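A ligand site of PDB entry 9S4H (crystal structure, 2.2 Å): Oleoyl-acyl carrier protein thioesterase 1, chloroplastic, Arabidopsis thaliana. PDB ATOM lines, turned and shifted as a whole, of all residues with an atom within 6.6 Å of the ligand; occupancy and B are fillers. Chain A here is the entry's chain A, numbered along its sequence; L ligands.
O1 of the ligand sits at hydrogen-bond distance from NE of Arg 103 (3.1 Å).
SG of Cys 93 sits at hydrogen-bond distance from O1 of the ligand (3.2 Å).
The guanidinium group of Arg 103 is in hydrogen-bond range of the side-chain sulfur of Cys 93 (3.1 Å).
The guanidinium group (NH2) of Arg 103 is in hydrogen-bond range of a ring nitrogen (ND1) of His 44 (3.1 Å).
O of Arg 103 is in hydrogen-bond range of N of Ser 121.
O of Cys 93 lies close to SG of Cys 148, at 3.6 Å.
The backbone NH (N) of Trp 123 sits at hydrogen-bond distance from the backbone carbonyl oxygen (O) of Thr 101, at 2.9 Å.
N of Trp 68 sits close to O of Phe 55 (3.4 Å).
OG of Ser 121 is in hydrogen-bond range of NE1 of Trp 123, 2.8 Å away.
The side-chain sulfur (SG) of Cys 148 sits at hydrogen-bond distance from the backbone carbonyl oxygen (O) of Tyr 144 (3.5 Å).
His 44 touches the ligand.
CA of Ala 45 touches C7 of the ligand, 3.8 Å away.
Val 48 touches the ligand (CG2 to C6, 3.8 Å).
Phe 50 touches the ligand.
CB of Ala 56 touches C4 of the ligand, 3.5 Å away.
NE1 of Trp 68 touches C9 of the ligand, at 3.3 Å.
OG1 of Thr 101 touches C10 of the ligand, 3.2 Å away.
Trp 123 touches the ligand.
Tyr 144 touches the ligand (CB to S1, 3.8 Å).
CB of Phe 147 touches C3 of the ligand, at 3.9 Å.
Within 4 Å of the ligand: His 44, Ala 45, Val 48, Phe 50, Ala 56, Trp 68, Cys 93, Thr 101, Arg 103, Trp 123, Tyr 144 and Phe 147.
The nearest printed residue that does not touch the ligand is Cys 148 (4.1 Å).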
ATOM      1  N   GLY A  41      20.476 -13.890  13.846  1.00  0.00           N
ATOM      2  CA  GLY A  41      20.676 -13.205  15.109  1.00  0.00           C
ATOM      3  C   GLY A  41      20.336 -11.727  15.008  1.00  0.00           C
ATOM      4  O   GLY A  41      19.638 -11.188  15.855  1.00  0.00           O
ATOM      5  N   HIS A  44      16.630 -11.210  14.767  1.00  0.00           N
ATOM      6  CA  HIS A  44      15.960 -11.512  16.017  1.00  0.00           C
ATOM      7  C   HIS A  44      16.045 -10.265  16.883  1.00  0.00           C
ATOM      8  O   HIS A  44      15.057  -9.894  17.517  1.00  0.00           O
ATOM      9  CB  HIS A  44      16.546 -12.767  16.677  1.00  0.00           C
ATOM     10  CG  HIS A  44      15.891 -13.052  17.979  1.00  0.00           C
ATOM     11  ND1 HIS A  44      16.459 -13.821  18.976  1.00  0.00           N
ATOM     12  CD2 HIS A  44      14.710 -12.649  18.480  1.00  0.00           C
ATOM     13  CE1 HIS A  44      15.640 -13.880  20.018  1.00  0.00           C
ATOM     14  NE2 HIS A  44      14.575 -13.174  19.734  1.00  0.00           N
ATOM     15  N   ALA A  45      17.195  -9.597  16.848  1.00  0.00           N
ATOM     16  CA  ALA A  45      17.421  -8.400  17.637  1.00  0.00           C
ATOM     17  C   ALA A  45      16.581  -7.228  17.141  1.00  0.00           C
ATOM     18  O   ALA A  45      16.099  -6.438  17.937  1.00  0.00           O
ATOM     19  CB  ALA A  45      18.901  -8.045  17.624  1.00  0.00           C
ATOM     20  N   GLN A  46      16.452  -7.111  15.804  1.00  0.00           N
ATOM     21  CA  GLN A  46      15.608  -6.104  15.172  1.00  0.00           C
ATOM     22  C   GLN A  46      14.170  -6.311  15.647  1.00  0.00           C
ATOM     23  O   GLN A  46      13.571  -5.429  16.262  1.00  0.00           O
ATOM     24  CB  GLN A  46      15.663  -6.241  13.649  1.00  0.00           C
ATOM     25  CG  GLN A  46      15.175  -5.012  12.878  1.00  0.00           C
ATOM     26  CD  GLN A  46      13.835  -4.489  13.323  1.00  0.00           C
ATOM     27  OE1 GLN A  46      13.709  -3.334  13.782  1.00  0.00           O
ATOM     28  NE2 GLN A  46      12.804  -5.317  13.204  1.00  0.00           N
ATOM     29  N   SER A  47      13.663  -7.522  15.400  1.00  0.00           N
ATOM     30  CA  SER A  47      12.265  -7.851  15.583  1.00  0.00           C
ATOM     31  C   SER A  47      11.782  -7.460  16.975  1.00  0.00           C
ATOM     32  O   SER A  47      10.565  -7.423  17.185  1.00  0.00           O
ATOM     33  CB  SER A  47      12.039  -9.318  15.353  1.00  0.00           C
ATOM     34  OG  SER A  47      12.692 -10.048  16.382  1.00  0.00           O
ATOM     35  N   VAL A  48      12.710  -7.165  17.899  1.00  0.00           N
ATOM     36  CA  VAL A  48      12.330  -6.836  19.273  1.00  0.00           C
ATOM     37  C   VAL A  48      12.867  -5.478  19.704  1.00  0.00           C
ATOM     38  O   VAL A  48      12.849  -5.176  20.897  1.00  0.00           O
ATOM     39  CB  VAL A  48      12.793  -7.951  20.244  1.00  0.00           C
ATOM     40  CG1 VAL A  48      11.975  -9.223  20.048  1.00  0.00           C
ATOM     41  CG2 VAL A  48      14.289  -8.229  20.134  1.00  0.00           C
ATOM     42  N   PHE A  50      16.120  -3.705  19.058  1.00  0.00           N
ATOM     43  CA  PHE A  50      17.518  -3.485  19.445  1.00  0.00           C
ATOM     44  C   PHE A  50      18.296  -2.933  18.243  1.00  0.00           C
ATOM     45  O   PHE A  50      17.712  -2.731  17.180  1.00  0.00           O
ATOM     46  CB  PHE A  50      18.159  -4.799  19.889  1.00  0.00           C
ATOM     47  CG  PHE A  50      17.673  -5.408  21.194  1.00  0.00           C
ATOM     48  CD1 PHE A  50      17.521  -4.634  22.335  1.00  0.00           C
ATOM     49  CD2 PHE A  50      17.363  -6.766  21.269  1.00  0.00           C
ATOM     50  CE1 PHE A  50      17.084  -5.205  23.514  1.00  0.00           C
ATOM     51  CE2 PHE A  50      16.924  -7.325  22.455  1.00  0.00           C
ATOM     52  CZ  PHE A  50      16.795  -6.546  23.577  1.00  0.00           C
ATOM     53  N   PHE A  55      25.322  -4.712  17.718  1.00  0.00           N
ATOM     54  CA  PHE A  55      25.741  -4.793  19.113  1.00  0.00           C
ATOM     55  C   PHE A  55      24.564  -5.111  20.041  1.00  0.00           C
ATOM     56  O   PHE A  55      24.776  -5.337  21.239  1.00  0.00           O
ATOM     57  CB  PHE A  55      26.383  -3.465  19.543  1.00  0.00           C
ATOM     58  CG  PHE A  55      27.661  -3.066  18.812  1.00  0.00           C
ATOM     59  CD1 PHE A  55      28.653  -3.995  18.529  1.00  0.00           C
ATOM     60  CD2 PHE A  55      27.885  -1.738  18.442  1.00  0.00           C
ATOM     61  CE1 PHE A  55      29.814  -3.616  17.864  1.00  0.00           C
ATOM     62  CE2 PHE A  55      29.040  -1.365  17.773  1.00  0.00           C
ATOM     63  CZ  PHE A  55      30.012  -2.304  17.485  1.00  0.00           C
ATOM     64  N   ALA A  56      23.340  -5.079  19.504  1.00  0.00           N
ATOM     65  CA  ALA A  56      22.135  -5.449  20.250  1.00  0.00           C
ATOM     66  C   ALA A  56      21.971  -4.603  21.515  1.00  0.00           C
ATOM     67  O   ALA A  56      21.685  -5.154  22.575  1.00  0.00           O
ATOM     68  CB  ALA A  56      22.210  -6.914  20.595  1.00  0.00           C
ATOM     69  N   THR A  57      22.088  -3.264  21.381  1.00  0.00           N
ATOM     70  CA  THR A  57      22.143  -2.372  22.529  1.00  0.00           C
ATOM     71  C   THR A  57      20.733  -1.943  22.914  1.00  0.00           C
ATOM     72  O   THR A  57      19.869  -1.820  22.051  1.00  0.00           O
ATOM     73  CB  THR A  57      23.031  -1.146  22.236  1.00  0.00           C
ATOM     74  OG1 THR A  57      22.565  -0.537  21.030  1.00  0.00           O
ATOM     75  CG2 THR A  57      24.484  -1.485  22.041  1.00  0.00           C
ATOM     76  N   TRP A  68      27.285  -5.671  23.564  1.00  0.00           N
ATOM     77  CA  TRP A  68      27.492  -7.099  23.485  1.00  0.00           C
ATOM     78  C   TRP A  68      28.602  -7.405  22.496  1.00  0.00           C
ATOM     79  O   TRP A  68      28.609  -6.831  21.408  1.00  0.00           O
ATOM     80  CB  TRP A  68      26.210  -7.835  23.072  1.00  0.00           C
ATOM     81  CG  TRP A  68      25.130  -7.751  24.121  1.00  0.00           C
ATOM     82  CD1 TRP A  68      23.974  -7.040  24.060  1.00  0.00           C
ATOM     83  CD2 TRP A  68      25.164  -8.393  25.411  1.00  0.00           C
ATOM     84  NE1 TRP A  68      23.266  -7.209  25.218  1.00  0.00           N
ATOM     85  CE2 TRP A  68      23.968  -8.025  26.062  1.00  0.00           C
ATOM     86  CE3 TRP A  68      26.077  -9.235  26.070  1.00  0.00           C
ATOM     87  CZ2 TRP A  68      23.662  -8.468  27.351  1.00  0.00           C
ATOM     88  CZ3 TRP A  68      25.772  -9.669  27.342  1.00  0.00           C
ATOM     89  CH2 TRP A  68      24.579  -9.305  27.968  1.00  0.00           C
ATOM     90  N   TRP A  92      17.591 -18.087  19.485  1.00  0.00           N
ATOM     91  CA  TRP A  92      17.083 -17.479  20.681  1.00  0.00           C
ATOM     92  C   TRP A  92      18.259 -17.230  21.622  1.00  0.00           C
ATOM     93  O   TRP A  92      19.339 -17.753  21.383  1.00  0.00           O
ATOM     94  CB  TRP A  92      16.038 -18.387  21.347  1.00  0.00           C
ATOM     95  CG  TRP A  92      16.655 -19.639  21.898  1.00  0.00           C
ATOM     96  CD1 TRP A  92      17.067 -19.864  23.179  1.00  0.00           C
ATOM     97  CD2 TRP A  92      16.968 -20.829  21.148  1.00  0.00           C
ATOM     98  NE1 TRP A  92      17.607 -21.118  23.282  1.00  0.00           N
ATOM     99  CE2 TRP A  92      17.559 -21.732  22.069  1.00  0.00           C
ATOM    100  CE3 TRP A  92      16.795 -21.223  19.817  1.00  0.00           C
ATOM    101  CZ2 TRP A  92      17.973 -23.007  21.680  1.00  0.00           C
ATOM    102  CZ3 TRP A  92      17.185 -22.486  19.444  1.00  0.00           C
ATOM    103  CH2 TRP A  92      17.772 -23.355  20.360  1.00  0.00           C
ATOM    104  N   CYS A  93      18.007 -16.458  22.682  1.00  0.00           N
ATOM    105  CA  CYS A  93      18.988 -16.129  23.701  1.00  0.00           C
ATOM    106  C   CYS A  93      18.518 -16.625  25.061  1.00  0.00           C
ATOM    107  O   CYS A  93      17.318 -16.781  25.266  1.00  0.00           O
ATOM    108  CB  CYS A  93      19.230 -14.623  23.774  1.00  0.00           C
ATOM    109  SG  CYS A  93      20.072 -13.954  22.318  1.00  0.00           S
ATOM    110  N   GLN A  94      19.452 -16.886  25.970  1.00  0.00           N
ATOM    111  CA  GLN A  94      19.151 -16.999  27.398  1.00  0.00           C
ATOM    112  C   GLN A  94      20.206 -16.257  28.198  1.00  0.00           C
ATOM    113  O   GLN A  94      21.297 -15.995  27.685  1.00  0.00           O
ATOM    114  CB  GLN A  94      19.071 -18.449  27.858  1.00  0.00           C
ATOM    115  CG  GLN A  94      17.893 -19.214  27.277  1.00  0.00           C
ATOM    116  CD  GLN A  94      17.489 -20.394  28.117  1.00  0.00           C
ATOM    117  OE1 GLN A  94      18.172 -21.421  28.145  1.00  0.00           O
ATOM    118  NE2 GLN A  94      16.375 -20.260  28.821  1.00  0.00           N
ATOM    119  N   THR A 101      25.161 -13.407  28.309  1.00  0.00           N
ATOM    120  CA  THR A 101      24.085 -14.146  27.677  1.00  0.00           C
ATOM    121  C   THR A 101      24.674 -15.194  26.747  1.00  0.00           C
ATOM    122  O   THR A 101      25.858 -15.182  26.437  1.00  0.00           O
ATOM    123  CB  THR A 101      23.169 -13.177  26.935  1.00  0.00           C
ATOM    124  OG1 THR A 101      23.927 -12.451  25.973  1.00  0.00           O
ATOM    125  CG2 THR A 101      22.476 -12.245  27.907  1.00  0.00           C
ATOM    126  N   ARG A 102      23.795 -16.101  26.316  1.00  0.00           N
ATOM    127  CA  ARG A 102      24.120 -17.151  25.379  1.00  0.00           C
ATOM    128  C   ARG A 102      23.133 -17.039  24.218  1.00  0.00           C
ATOM    129  O   ARG A 102      21.942 -16.874  24.435  1.00  0.00           O
ATOM    130  CB  ARG A 102      23.994 -18.482  26.118  1.00  0.00           C
ATOM    131  CG  ARG A 102      24.584 -19.673  25.385  1.00  0.00           C
ATOM    132  CD  ARG A 102      24.199 -21.019  25.999  1.00  0.00           C
ATOM    133  NE  ARG A 102      22.787 -21.344  25.760  1.00  0.00           N
ATOM    134  CZ  ARG A 102      21.790 -21.414  26.647  1.00  0.00           C
ATOM    135  NH1 ARG A 102      20.549 -21.539  26.199  1.00  0.00           N
ATOM    136  NH2 ARG A 102      22.014 -21.298  27.945  1.00  0.00           N
ATOM    137  N   ARG A 103      23.630 -17.073  22.978  1.00  0.00           N
ATOM    138  CA  ARG A 103      22.717 -17.236  21.852  1.00  0.00           C
ATOM    139  C   ARG A 103      22.916 -18.632  21.310  1.00  0.00           C
ATOM    140  O   ARG A 103      24.014 -19.181  21.393  1.00  0.00           O
ATOM    141  CB  ARG A 103      22.872 -16.144  20.797  1.00  0.00           C
ATOM    142  CG  ARG A 103      22.003 -16.357  19.559  1.00  0.00           C
ATOM    143  CD  ARG A 103      22.107 -15.170  18.616  1.00  0.00           C
ATOM    144  NE  ARG A 103      21.317 -14.023  19.077  1.00  0.00           N
ATOM    145  CZ  ARG A 103      20.003 -13.927  19.002  1.00  0.00           C
ATOM    146  NH1 ARG A 103      19.400 -12.849  19.457  1.00  0.00           N
ATOM    147  NH2 ARG A 103      19.305 -14.912  18.482  1.00  0.00           N
ATOM    148  N   SER A 121      26.899 -19.768  21.546  1.00  0.00           N
ATOM    149  CA  SER A 121      27.805 -18.634  21.598  1.00  0.00           C
ATOM    150  C   SER A 121      27.684 -17.972  22.964  1.00  0.00           C
ATOM    151  O   SER A 121      26.602 -17.957  23.545  1.00  0.00           O
ATOM    152  CB  SER A 121      27.504 -17.642  20.494  1.00  0.00           C
ATOM    153  OG  SER A 121      26.206 -17.097  20.661  1.00  0.00           O
ATOM    154  N   TRP A 123      28.125 -14.360  24.825  1.00  0.00           N
ATOM    155  CA  TRP A 123      28.224 -12.921  24.660  1.00  0.00           C
ATOM    156  C   TRP A 123      28.479 -12.290  26.021  1.00  0.00           C
ATOM    157  O   TRP A 123      28.048 -12.803  27.050  1.00  0.00           O
ATOM    158  CB  TRP A 123      26.947 -12.383  24.012  1.00  0.00           C
ATOM    159  CG  TRP A 123      26.737 -12.893  22.612  1.00  0.00           C
ATOM    160  CD1 TRP A 123      26.328 -14.139  22.273  1.00  0.00           C
ATOM    161  CD2 TRP A 123      26.935 -12.184  21.360  1.00  0.00           C
ATOM    162  NE1 TRP A 123      26.253 -14.263  20.909  1.00  0.00           N
ATOM    163  CE2 TRP A 123      26.613 -13.080  20.326  1.00  0.00           C
ATOM    164  CE3 TRP A 123      27.340 -10.891  21.010  1.00  0.00           C
ATOM    165  CZ2 TRP A 123      26.694 -12.737  18.971  1.00  0.00           C
ATOM    166  CZ3 TRP A 123      27.410 -10.539  19.681  1.00  0.00           C
ATOM    167  CH2 TRP A 123      27.096 -11.453  18.671  1.00  0.00           C
ATOM    168  N   TYR A 144      16.422  -7.250  28.699  1.00  0.00           N
ATOM    169  CA  TYR A 144      16.481  -8.289  27.682  1.00  0.00           C
ATOM    170  C   TYR A 144      15.752  -9.558  28.103  1.00  0.00           C
ATOM    171  O   TYR A 144      15.373 -10.337  27.235  1.00  0.00           O
ATOM    172  CB  TYR A 144      17.923  -8.531  27.233  1.00  0.00           C
ATOM    173  CG  TYR A 144      18.943  -9.118  28.207  1.00  0.00           C
ATOM    174  CD1 TYR A 144      18.869 -10.441  28.651  1.00  0.00           C
ATOM    175  CD2 TYR A 144      20.053  -8.374  28.609  1.00  0.00           C
ATOM    176  CE1 TYR A 144      19.830 -10.981  29.491  1.00  0.00           C
ATOM    177  CE2 TYR A 144      21.017  -8.898  29.468  1.00  0.00           C
ATOM    178  CZ  TYR A 144      20.913 -10.212  29.916  1.00  0.00           C
ATOM    179  OH  TYR A 144      21.887 -10.729  30.745  1.00  0.00           O
ATOM    180  N   LEU A 145      15.478  -9.738  29.399  1.00  0.00           N
ATOM    181  CA  LEU A 145      14.941 -11.005  29.914  1.00  0.00           C
ATOM    182  C   LEU A 145      13.580 -11.342  29.338  1.00  0.00           C
ATOM    183  O   LEU A 145      13.209 -12.516  29.290  1.00  0.00           O
ATOM    184  CB  LEU A 145      14.857 -10.988  31.445  1.00  0.00           C
ATOM    185  CG  LEU A 145      16.105 -11.511  32.167  1.00  0.00           C
ATOM    186  CD1 LEU A 145      16.302 -13.009  31.965  1.00  0.00           C
ATOM    187  CD2 LEU A 145      17.301 -10.757  31.641  1.00  0.00           C
ATOM    188  N   PHE A 147      12.708 -11.126  26.439  1.00  0.00           N
ATOM    189  CA  PHE A 147      12.887 -11.632  25.084  1.00  0.00           C
ATOM    190  C   PHE A 147      13.489 -13.040  25.114  1.00  0.00           C
ATOM    191  O   PHE A 147      13.745 -13.626  24.066  1.00  0.00           O
ATOM    192  CB  PHE A 147      13.694 -10.604  24.270  1.00  0.00           C
ATOM    193  CG  PHE A 147      13.049  -9.224  24.281  1.00  0.00           C
ATOM    194  CD1 PHE A 147      11.822  -8.998  23.670  1.00  0.00           C
ATOM    195  CD2 PHE A 147      13.683  -8.145  24.912  1.00  0.00           C
ATOM    196  CE1 PHE A 147      11.240  -7.732  23.694  1.00  0.00           C
ATOM    197  CE2 PHE A 147      13.095  -6.887  24.932  1.00  0.00           C
ATOM    198  CZ  PHE A 147      11.870  -6.678  24.324  1.00  0.00           C
ATOM    199  N   CYS A 148      13.647 -13.592  26.328  1.00  0.00           N
ATOM    200  CA  CYS A 148      14.264 -14.892  26.534  1.00  0.00           C
ATOM    201  C   CYS A 148      13.277 -15.800  27.268  1.00  0.00           C
ATOM    202  O   CYS A 148      12.461 -15.296  28.050  1.00  0.00           O
ATOM    203  CB  CYS A 148      15.525 -14.808  27.385  1.00  0.00           C
ATOM    204  SG  CYS A 148      16.708 -13.545  26.839  1.00  0.00           S
HETATM  205  C1  LIG L   1      20.953 -10.863  25.148  1.00  0.00           C
HETATM  206  C2  LIG L   1      18.516 -10.883  23.152  1.00  0.00           C
HETATM  207  C3  LIG L   1      17.239 -11.438  23.006  1.00  0.00           C
HETATM  208  C4  LIG L   1      20.457  -9.577  22.135  1.00  0.00           C
HETATM  209  C5  LIG L   1      16.567 -11.358  21.804  1.00  0.00           C
HETATM  210  C6  LIG L   1      17.145 -10.718  20.728  1.00  0.00           C
HETATM  211  C7  LIG L   1      18.396 -10.175  20.857  1.00  0.00           C
HETATM  212  C8  LIG L   1      19.111 -10.241  22.045  1.00  0.00           C
HETATM  213  N1  LIG L   1      21.499 -10.362  22.803  1.00  0.00           N
HETATM  214  C9  LIG L   1      21.725  -9.974  24.199  1.00  0.00           C
HETATM  215  C10 LIG L   1      23.314 -11.991  22.855  1.00  0.00           C
HETATM  216  C11 LIG L   1      22.172 -11.309  22.168  1.00  0.00           C
HETATM  217  O1  LIG L   1      21.843 -11.616  21.031  1.00  0.00           O
HETATM  218  S1  LIG L   1      19.194 -11.073  24.780  1.00  0.00           S
